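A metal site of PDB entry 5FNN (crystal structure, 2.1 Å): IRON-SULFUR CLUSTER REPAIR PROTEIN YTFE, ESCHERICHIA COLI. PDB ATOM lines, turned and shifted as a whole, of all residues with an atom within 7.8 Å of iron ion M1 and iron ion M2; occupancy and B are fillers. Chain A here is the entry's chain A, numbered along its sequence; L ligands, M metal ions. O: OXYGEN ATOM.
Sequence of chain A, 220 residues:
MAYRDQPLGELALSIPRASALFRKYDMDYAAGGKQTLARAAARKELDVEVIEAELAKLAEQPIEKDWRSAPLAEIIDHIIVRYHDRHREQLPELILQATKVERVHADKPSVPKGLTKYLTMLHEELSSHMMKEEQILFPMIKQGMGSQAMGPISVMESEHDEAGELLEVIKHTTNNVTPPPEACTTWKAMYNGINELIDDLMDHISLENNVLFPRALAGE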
ATOM      1  N   ILE A  79      33.485   5.438  -0.784  1.00  0.00           N
ATOM      2  CA  ILE A  79      32.593   4.928   0.248  1.00  0.00           C
ATOM      3  C   ILE A  79      32.714   3.418   0.372  1.00  0.00           C
ATOM      4  O   ILE A  79      32.840   2.888   1.481  1.00  0.00           O
ATOM      5  CB  ILE A  79      31.135   5.313  -0.012  1.00  0.00           C
ATOM      6  CG1 ILE A  79      30.930   6.805   0.243  1.00  0.00           C
ATOM      7  CG2 ILE A  79      30.202   4.485   0.867  1.00  0.00           C
ATOM      8  CD1 ILE A  79      29.612   7.344  -0.253  1.00  0.00           C
ATOM      9  N   ILE A  80      32.674   2.713  -0.755  1.00  0.00           N
ATOM     10  CA  ILE A  80      32.741   1.236  -0.738  1.00  0.00           C
ATOM     11  C   ILE A  80      34.013   0.749  -0.062  1.00  0.00           C
ATOM     12  O   ILE A  80      33.960  -0.157   0.767  1.00  0.00           O
ATOM     13  CB  ILE A  80      32.622   0.637  -2.136  1.00  0.00           C
ATOM     14  CG1 ILE A  80      31.204   0.806  -2.672  1.00  0.00           C
ATOM     15  CG2 ILE A  80      32.961  -0.843  -2.143  1.00  0.00           C
ATOM     16  CD1 ILE A  80      31.088   0.608  -4.189  1.00  0.00           C
ATOM     17  N   TYR A  83      34.833   3.006   3.692  1.00  0.00           N
ATOM     18  CA  TYR A  83      33.819   2.789   4.727  1.00  0.00           C
ATOM     19  C   TYR A  83      33.175   1.399   4.724  1.00  0.00           C
ATOM     20  O   TYR A  83      33.300   0.687   5.713  1.00  0.00           O
ATOM     21  CB  TYR A  83      32.778   3.916   4.672  1.00  0.00           C
ATOM     22  CG  TYR A  83      33.416   5.256   4.962  1.00  0.00           C
ATOM     23  CD1 TYR A  83      34.086   5.496   6.155  1.00  0.00           C
ATOM     24  CD2 TYR A  83      33.365   6.290   4.045  1.00  0.00           C
ATOM     25  CE1 TYR A  83      34.682   6.720   6.434  1.00  0.00           C
ATOM     26  CE2 TYR A  83      33.959   7.525   4.315  1.00  0.00           C
ATOM     27  CZ  TYR A  83      34.616   7.725   5.508  1.00  0.00           C
ATOM     28  OH  TYR A  83      35.174   8.941   5.805  1.00  0.00           O
ATOM     29  N   HIS A  84      32.517   0.981   3.635  1.00  0.00           N
ATOM     30  CA  HIS A  84      31.782  -0.303   3.694  1.00  0.00           C
ATOM     31  C   HIS A  84      32.680  -1.487   4.025  1.00  0.00           C
ATOM     32  O   HIS A  84      32.377  -2.265   4.934  1.00  0.00           O
ATOM     33  CB  HIS A  84      31.030  -0.639   2.407  1.00  0.00           C
ATOM     34  CG  HIS A  84      29.872   0.243   2.121  1.00  0.00           C
ATOM     35  ND1 HIS A  84      28.989  -0.017   1.079  1.00  0.00           N
ATOM     36  CD2 HIS A  84      29.450   1.391   2.696  1.00  0.00           C
ATOM     37  CE1 HIS A  84      28.037   0.898   1.077  1.00  0.00           C
ATOM     38  NE2 HIS A  84      28.306   1.774   2.031  1.00  0.00           N
ATOM     39  N   HIS A  87      33.839  -1.357   7.640  1.00  0.00           N
ATOM     40  CA  HIS A  87      32.809  -1.760   8.622  1.00  0.00           C
ATOM     41  C   HIS A  87      32.652  -3.276   8.626  1.00  0.00           C
ATOM     42  O   HIS A  87      32.487  -3.874   9.663  1.00  0.00           O
ATOM     43  CB  HIS A  87      31.444  -1.140   8.330  1.00  0.00           C
ATOM     44  CG  HIS A  87      31.428   0.354   8.303  1.00  0.00           C
ATOM     45  ND1 HIS A  87      32.230   1.120   9.110  1.00  0.00           N
ATOM     46  CD2 HIS A  87      30.632   1.228   7.642  1.00  0.00           C
ATOM     47  CE1 HIS A  87      31.955   2.406   8.930  1.00  0.00           C
ATOM     48  NE2 HIS A  87      30.990   2.497   8.032  1.00  0.00           N
ATOM     49  N   LEU A 126      23.507  -3.017   9.091  1.00  0.00           N
ATOM     50  CA  LEU A 126      24.445  -2.398   8.172  1.00  0.00           C
ATOM     51  C   LEU A 126      24.735  -3.280   6.972  1.00  0.00           C
ATOM     52  O   LEU A 126      24.857  -2.782   5.832  1.00  0.00           O
ATOM     53  CB  LEU A 126      25.793  -2.106   8.828  1.00  0.00           C
ATOM     54  CG  LEU A 126      26.232  -0.724   9.219  1.00  0.00           C
ATOM     55  CD1 LEU A 126      27.726  -0.768   9.604  1.00  0.00           C
ATOM     56  CD2 LEU A 126      25.983   0.289   8.132  1.00  0.00           C
ATOM     57  N   HIS A 129      21.839  -3.229   4.557  1.00  0.00           N
ATOM     58  CA  HIS A 129      21.774  -1.851   4.067  1.00  0.00           C
ATOM     59  C   HIS A 129      22.858  -1.599   3.018  1.00  0.00           C
ATOM     60  O   HIS A 129      22.550  -1.143   1.904  1.00  0.00           O
ATOM     61  CB  HIS A 129      21.876  -0.893   5.243  1.00  0.00           C
ATOM     62  CG  HIS A 129      22.069   0.544   4.862  1.00  0.00           C
ATOM     63  ND1 HIS A 129      21.026   1.445   4.746  1.00  0.00           N
ATOM     64  CD2 HIS A 129      23.201   1.250   4.626  1.00  0.00           C
ATOM     65  CE1 HIS A 129      21.507   2.628   4.440  1.00  0.00           C
ATOM     66  NE2 HIS A 129      22.827   2.550   4.378  1.00  0.00           N
ATOM     67  N   MET A 130      24.101  -1.918   3.345  1.00  0.00           N
ATOM     68  CA  MET A 130      25.233  -1.720   2.424  1.00  0.00           C
ATOM     69  C   MET A 130      25.129  -2.530   1.149  1.00  0.00           C
ATOM     70  O   MET A 130      25.536  -2.053   0.084  1.00  0.00           O
ATOM     71  CB  MET A 130      26.547  -2.059   3.094  1.00  0.00           C
ATOM     72  CG  MET A 130      26.892  -0.984   4.130  1.00  0.00           C
ATOM     73  SD  MET A 130      28.631  -1.396   5.001  1.00  0.00           S
ATOM     74  CE  MET A 130      28.381  -3.275   5.583  1.00  0.00           C
ATOM     75  N   MET A 131      24.562  -3.731   1.237  1.00  0.00           N
ATOM     76  CA  MET A 131      24.363  -4.589   0.051  1.00  0.00           C
ATOM     77  C   MET A 131      23.401  -3.970  -0.914  1.00  0.00           C
ATOM     78  O   MET A 131      23.639  -4.001  -2.128  1.00  0.00           O
ATOM     79  CB  MET A 131      23.824  -5.974   0.436  1.00  0.00           C
ATOM     80  CG  MET A 131      23.452  -6.874  -0.764  1.00  0.00           C
ATOM     81  SD  MET A 131      22.835  -8.632  -0.115  1.00  0.00           S
ATOM     82  CE  MET A 131      24.581  -9.322   0.534  1.00  0.00           C
ATOM     83  N   GLU A 133      22.801  -0.697  -1.148  1.00  0.00           N
ATOM     84  CA  GLU A 133      23.508   0.444  -1.739  1.00  0.00           C
ATOM     85  C   GLU A 133      24.416  -0.048  -2.854  1.00  0.00           C
ATOM     86  O   GLU A 133      24.410   0.510  -3.948  1.00  0.00           O
ATOM     87  CB  GLU A 133      24.301   1.276  -0.696  1.00  0.00           C
ATOM     88  CG  GLU A 133      23.398   1.999   0.284  1.00  0.00           C
ATOM     89  CD  GLU A 133      24.112   2.922   1.270  1.00  0.00           C
ATOM     90  OE1 GLU A 133      25.299   2.644   1.656  1.00  0.00           O
ATOM     91  OE2 GLU A 133      23.438   3.922   1.705  1.00  0.00           O
ATOM     92  N   GLU A 134      25.173  -1.103  -2.592  1.00  0.00           N
ATOM     93  CA  GLU A 134      26.160  -1.582  -3.560  1.00  0.00           C
ATOM     94  C   GLU A 134      25.549  -2.257  -4.796  1.00  0.00           C
ATOM     95  O   GLU A 134      26.137  -2.167  -5.886  1.00  0.00           O
ATOM     96  CB  GLU A 134      27.164  -2.525  -2.912  1.00  0.00           C
ATOM     97  CG  GLU A 134      28.214  -1.793  -2.094  1.00  0.00           C
ATOM     98  CD  GLU A 134      29.113  -2.706  -1.296  1.00  0.00           C
ATOM     99  OE1 GLU A 134      29.304  -3.863  -1.713  1.00  0.00           O
ATOM    100  OE2 GLU A 134      29.619  -2.281  -0.243  1.00  0.00           O
ATOM    101  N   LEU A 137      21.523   1.079  -5.555  1.00  0.00           N
ATOM    102  CA  LEU A 137      21.570   2.543  -5.527  1.00  0.00           C
ATOM    103  C   LEU A 137      22.831   3.151  -6.132  1.00  0.00           C
ATOM    104  O   LEU A 137      22.758   4.106  -6.906  1.00  0.00           O
ATOM    105  CB  LEU A 137      21.386   3.089  -4.125  1.00  0.00           C
ATOM    106  CG  LEU A 137      21.490   4.598  -3.962  1.00  0.00           C
ATOM    107  CD1 LEU A 137      20.451   5.316  -4.807  1.00  0.00           C
ATOM    108  CD2 LEU A 137      21.295   4.981  -2.510  1.00  0.00           C
ATOM    109  N   PHE A 138      23.987   2.614  -5.753  1.00  0.00           N
ATOM    110  CA  PHE A 138      25.262   3.076  -6.302  1.00  0.00           C
ATOM    111  C   PHE A 138      25.375   2.858  -7.844  1.00  0.00           C
ATOM    112  O   PHE A 138      25.667   3.825  -8.559  1.00  0.00           O
ATOM    113  CB  PHE A 138      26.438   2.480  -5.520  1.00  0.00           C
ATOM    114  CG  PHE A 138      26.590   3.024  -4.094  1.00  0.00           C
ATOM    115  CD1 PHE A 138      25.841   4.108  -3.612  1.00  0.00           C
ATOM    116  CD2 PHE A 138      27.537   2.476  -3.253  1.00  0.00           C
ATOM    117  CE1 PHE A 138      26.003   4.570  -2.330  1.00  0.00           C
ATOM    118  CE2 PHE A 138      27.729   2.966  -1.985  1.00  0.00           C
ATOM    119  CZ  PHE A 138      26.954   4.003  -1.513  1.00  0.00           C
ATOM    120  N   MET A 156      17.086   4.608   2.404  1.00  0.00           N
ATOM    121  CA  MET A 156      18.458   4.645   2.939  1.00  0.00           C
ATOM    122  C   MET A 156      18.586   5.643   4.081  1.00  0.00           C
ATOM    123  O   MET A 156      19.262   5.382   5.074  1.00  0.00           O
ATOM    124  CB  MET A 156      19.538   5.027   1.913  1.00  0.00           C
ATOM    125  CG  MET A 156      19.758   4.058   0.752  1.00  0.00           C
ATOM    126  SD  MET A 156      19.972   2.187   1.328  1.00  0.00           S
ATOM    127  CE  MET A 156      18.143   1.614   0.864  1.00  0.00           C
ATOM    128  N   GLU A 157      17.937   6.801   3.937  1.00  0.00           N
ATOM    129  CA  GLU A 157      17.987   7.841   4.998  1.00  0.00           C
ATOM    130  C   GLU A 157      17.252   7.442   6.261  1.00  0.00           C
ATOM    131  O   GLU A 157      17.738   7.704   7.366  1.00  0.00           O
ATOM    132  CB  GLU A 157      17.534   9.207   4.486  1.00  0.00           C
ATOM    133  CG  GLU A 157      18.571   9.838   3.544  1.00  0.00           C
ATOM    134  CD  GLU A 157      18.215  11.262   3.075  1.00  0.00           C
ATOM    135  OE1 GLU A 157      17.064  11.707   3.295  1.00  0.00           O
ATOM    136  OE2 GLU A 157      19.090  11.936   2.474  1.00  0.00           O
ATOM    137  N   GLU A 159      17.000   4.368   7.251  1.00  0.00           N
ATOM    138  CA  GLU A 159      17.954   3.384   7.834  1.00  0.00           C
ATOM    139  C   GLU A 159      19.179   4.001   8.477  1.00  0.00           C
ATOM    140  O   GLU A 159      19.607   3.538   9.530  1.00  0.00           O
ATOM    141  CB  GLU A 159      18.332   2.332   6.794  1.00  0.00           C
ATOM    142  CG  GLU A 159      17.124   1.439   6.484  1.00  0.00           C
ATOM    143  CD  GLU A 159      17.379   0.422   5.394  1.00  0.00           C
ATOM    144  OE1 GLU A 159      18.482   0.400   4.801  1.00  0.00           O
ATOM    145  OE2 GLU A 159      16.474  -0.369   5.104  1.00  0.00           O
ATOM    146  N   HIS A 160      19.688   5.108   7.930  1.00  0.00           N
ATOM    147  CA  HIS A 160      20.747   5.870   8.604  1.00  0.00           C
ATOM    148  C   HIS A 160      20.325   6.391   9.968  1.00  0.00           C
ATOM    149  O   HIS A 160      21.146   6.373  10.886  1.00  0.00           O
ATOM    150  CB  HIS A 160      21.190   7.081   7.793  1.00  0.00           C
ATOM    151  CG  HIS A 160      21.889   6.718   6.542  1.00  0.00           C
ATOM    152  ND1 HIS A 160      22.136   7.619   5.533  1.00  0.00           N
ATOM    153  CD2 HIS A 160      22.340   5.518   6.101  1.00  0.00           C
ATOM    154  CE1 HIS A 160      22.720   6.999   4.524  1.00  0.00           C
ATOM    155  NE2 HIS A 160      22.854   5.727   4.842  1.00  0.00           N
ATOM    156  N   LEU A 201      31.506   5.689  10.713  1.00  0.00           N
ATOM    157  CA  LEU A 201      30.116   5.562  10.340  1.00  0.00           C
ATOM    158  C   LEU A 201      29.424   6.935  10.204  1.00  0.00           C
ATOM    159  O   LEU A 201      28.610   7.132   9.300  1.00  0.00           O
ATOM    160  CB  LEU A 201      29.412   4.616  11.309  1.00  0.00           C
ATOM    161  CG  LEU A 201      28.031   4.083  10.979  1.00  0.00           C
ATOM    162  CD1 LEU A 201      27.852   3.582   9.553  1.00  0.00           C
ATOM    163  CD2 LEU A 201      27.714   2.968  11.975  1.00  0.00           C
ATOM    164  N   HIS A 204      30.832   8.461   6.986  1.00  0.00           N
ATOM    165  CA  HIS A 204      30.174   7.667   5.935  1.00  0.00           C
ATOM    166  C   HIS A 204      28.744   8.189   5.702  1.00  0.00           C
ATOM    167  O   HIS A 204      28.401   8.598   4.592  1.00  0.00           O
ATOM    168  CB  HIS A 204      30.214   6.193   6.392  1.00  0.00           C
ATOM    169  CG  HIS A 204      29.446   5.246   5.529  1.00  0.00           C
ATOM    170  ND1 HIS A 204      29.126   3.970   5.934  1.00  0.00           N
ATOM    171  CD2 HIS A 204      28.883   5.401   4.315  1.00  0.00           C
ATOM    172  CE1 HIS A 204      28.418   3.375   4.996  1.00  0.00           C
ATOM    173  NE2 HIS A 204      28.253   4.223   4.007  1.00  0.00           N
ATOM    174  N   ILE A 205      27.931   8.223   6.764  1.00  0.00           N
ATOM    175  CA  ILE A 205      26.550   8.681   6.668  1.00  0.00           C
ATOM    176  C   ILE A 205      26.494  10.158   6.184  1.00  0.00           C
ATOM    177  O   ILE A 205      25.648  10.515   5.354  1.00  0.00           O
ATOM    178  CB  ILE A 205      25.759   8.544   7.998  1.00  0.00           C
ATOM    179  CG1 ILE A 205      25.566   7.090   8.470  1.00  0.00           C
ATOM    180  CG2 ILE A 205      24.395   9.239   7.940  1.00  0.00           C
ATOM    181  CD1 ILE A 205      25.412   6.080   7.394  1.00  0.00           C
ATOM    182  N   GLU A 208      27.088  10.424   2.478  1.00  0.00           N
ATOM    183  CA  GLU A 208      25.893  10.010   1.774  1.00  0.00           C
ATOM    184  C   GLU A 208      24.740  11.046   1.882  1.00  0.00           C
ATOM    185  O   GLU A 208      24.246  11.525   0.846  1.00  0.00           O
ATOM    186  CB  GLU A 208      25.452   8.604   2.186  1.00  0.00           C
ATOM    187  CG  GLU A 208      26.448   7.548   1.690  1.00  0.00           C
ATOM    188  CD  GLU A 208      26.158   6.125   2.136  1.00  0.00           C
ATOM    189  OE1 GLU A 208      25.189   5.872   2.900  1.00  0.00           O
ATOM    190  OE2 GLU A 208      26.991   5.244   1.808  1.00  0.00           O
ATOM    191  N   ASN A 209      24.386  11.429   3.104  1.00  0.00           N
ATOM    192  CA  ASN A 209      23.266  12.353   3.339  1.00  0.00           C
ATOM    193  C   ASN A 209      23.521  13.773   2.839  1.00  0.00           C
ATOM    194  O   ASN A 209      22.604  14.398   2.308  1.00  0.00           O
ATOM    195  CB  ASN A 209      22.889  12.409   4.826  1.00  0.00           C
ATOM    196  CG  ASN A 209      22.042  11.229   5.281  1.00  0.00           C
ATOM    197  OD1 ASN A 209      22.007  10.187   4.660  1.00  0.00           O
ATOM    198  ND2 ASN A 209      21.355  11.399   6.388  1.00  0.00           N
ATOM    199  N   LEU A 212      26.397  12.897  -1.562  1.00  0.00           N
ATOM    200  CA  LEU A 212      26.027  11.955  -2.611  1.00  0.00           C
ATOM    201  C   LEU A 212      24.551  11.986  -2.960  1.00  0.00           C
ATOM    202  O   LEU A 212      24.200  12.109  -4.145  1.00  0.00           O
ATOM    203  CB  LEU A 212      26.432  10.526  -2.278  1.00  0.00           C
ATOM    204  CG  LEU A 212      26.103   9.471  -3.337  1.00  0.00           C
ATOM    205  CD1 LEU A 212      26.860   9.740  -4.637  1.00  0.00           C
ATOM    206  CD2 LEU A 212      26.453   8.085  -2.822  1.00  0.00           C
ATOM    207  N   PHE A 213      23.692  11.857  -1.954  1.00  0.00           N
ATOM    208  CA  PHE A 213      22.262  11.763  -2.160  1.00  0.00           C
ATOM    209  C   PHE A 213      21.602  13.051  -2.734  1.00  0.00           C
ATOM    210  O   PHE A 213      20.856  12.954  -3.691  1.00  0.00           O
ATOM    211  CB  PHE A 213      21.535  11.291  -0.885  1.00  0.00           C
ATOM    212  CG  PHE A 213      21.861   9.852  -0.452  1.00  0.00           C
ATOM    213  CD1 PHE A 213      22.589   8.963  -1.251  1.00  0.00           C
ATOM    214  CD2 PHE A 213      21.378   9.382   0.765  1.00  0.00           C
ATOM    215  CE1 PHE A 213      22.852   7.671  -0.821  1.00  0.00           C
ATOM    216  CE2 PHE A 213      21.641   8.080   1.194  1.00  0.00           C
ATOM    217  CZ  PHE A 213      22.375   7.230   0.408  1.00  0.00           C
HETATM  218  O     O L   1      25.568   3.292   4.208  1.00  0.00           O
HETATM  219 FE    FE M   1      24.063   4.247   3.619  1.00  0.00          FE
HETATM  220 FE    FE M   2      26.811   3.411   2.666  1.00  0.00          FE
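O of Glu 133 sits at hydrogen-bond distance from N of Phe 138, at 2.8 Å. N of Phe 213 is in hydrogen-bond range of O of Glu 208, 2.9 Å away. A ring nitrogen (ND1) of His 204 lies within hydrogen-bond range of a ring nitrogen (NE2) of His 87 (3.2 Å). ND1 of His 129 lies close to SD of Met 156 (3.7 Å). OE1 of Glu 159 lies within hydrogen-bond range of ND1 of His 129. A ring nitrogen (ND1) of His 160 is in hydrogen-bond range of the side-chain amide oxygen (OD1) of Asn 209, at 2.7 Å. N of His 84 sits at hydrogen-bond distance from O of Ile 79, at 2.9 Å. A ring nitrogen (ND1) of His 84 sits at hydrogen-bond distance from the side-chain carboxylate (OE2) of Glu 134, at 2.7 Å.
Four residues have an atom within 4 Å of iron ion M1: His 129, Glu 133, His 160 and Glu 208. The nearest printed residue that does not touch iron ion M1 is His 204 (4.2 Å).
Residues that only touch iron ion M2: Ile 79 (3.99 Å). Within 4 Å of iron ion M2: Ile 79, His 84, Glu 133, His 204 and Glu 208. The nearest printed residue that does not touch iron ion M2 is Phe 138 (4.2 Å).
Iron ion M1 is bound by O of the ligand (1.9 Å). OE2 of Glu 133 is bound to iron ion M1 (2.0 Å). The side-chain carboxylate (OE1) of Glu 208 is bound to iron ion M1 (2.1 Å). A ring nitrogen (NE2) of His 129 is bound to iron ion M1. Iron ion M1 is bound by NE2 of His 160 (2.3 Å). Slightly farther from iron ion M1 lies OE1 of Glu 133 (2.8 Å).
Iron ion M2 is bound by OE1 of Glu 133 (2.0 Å), O of the ligand (2.0 Å), OE2 of Glu 208 (2.0 Å), NE2 of His 204 (2.1 Å) and NE2 of His 84 (2.3 Å).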
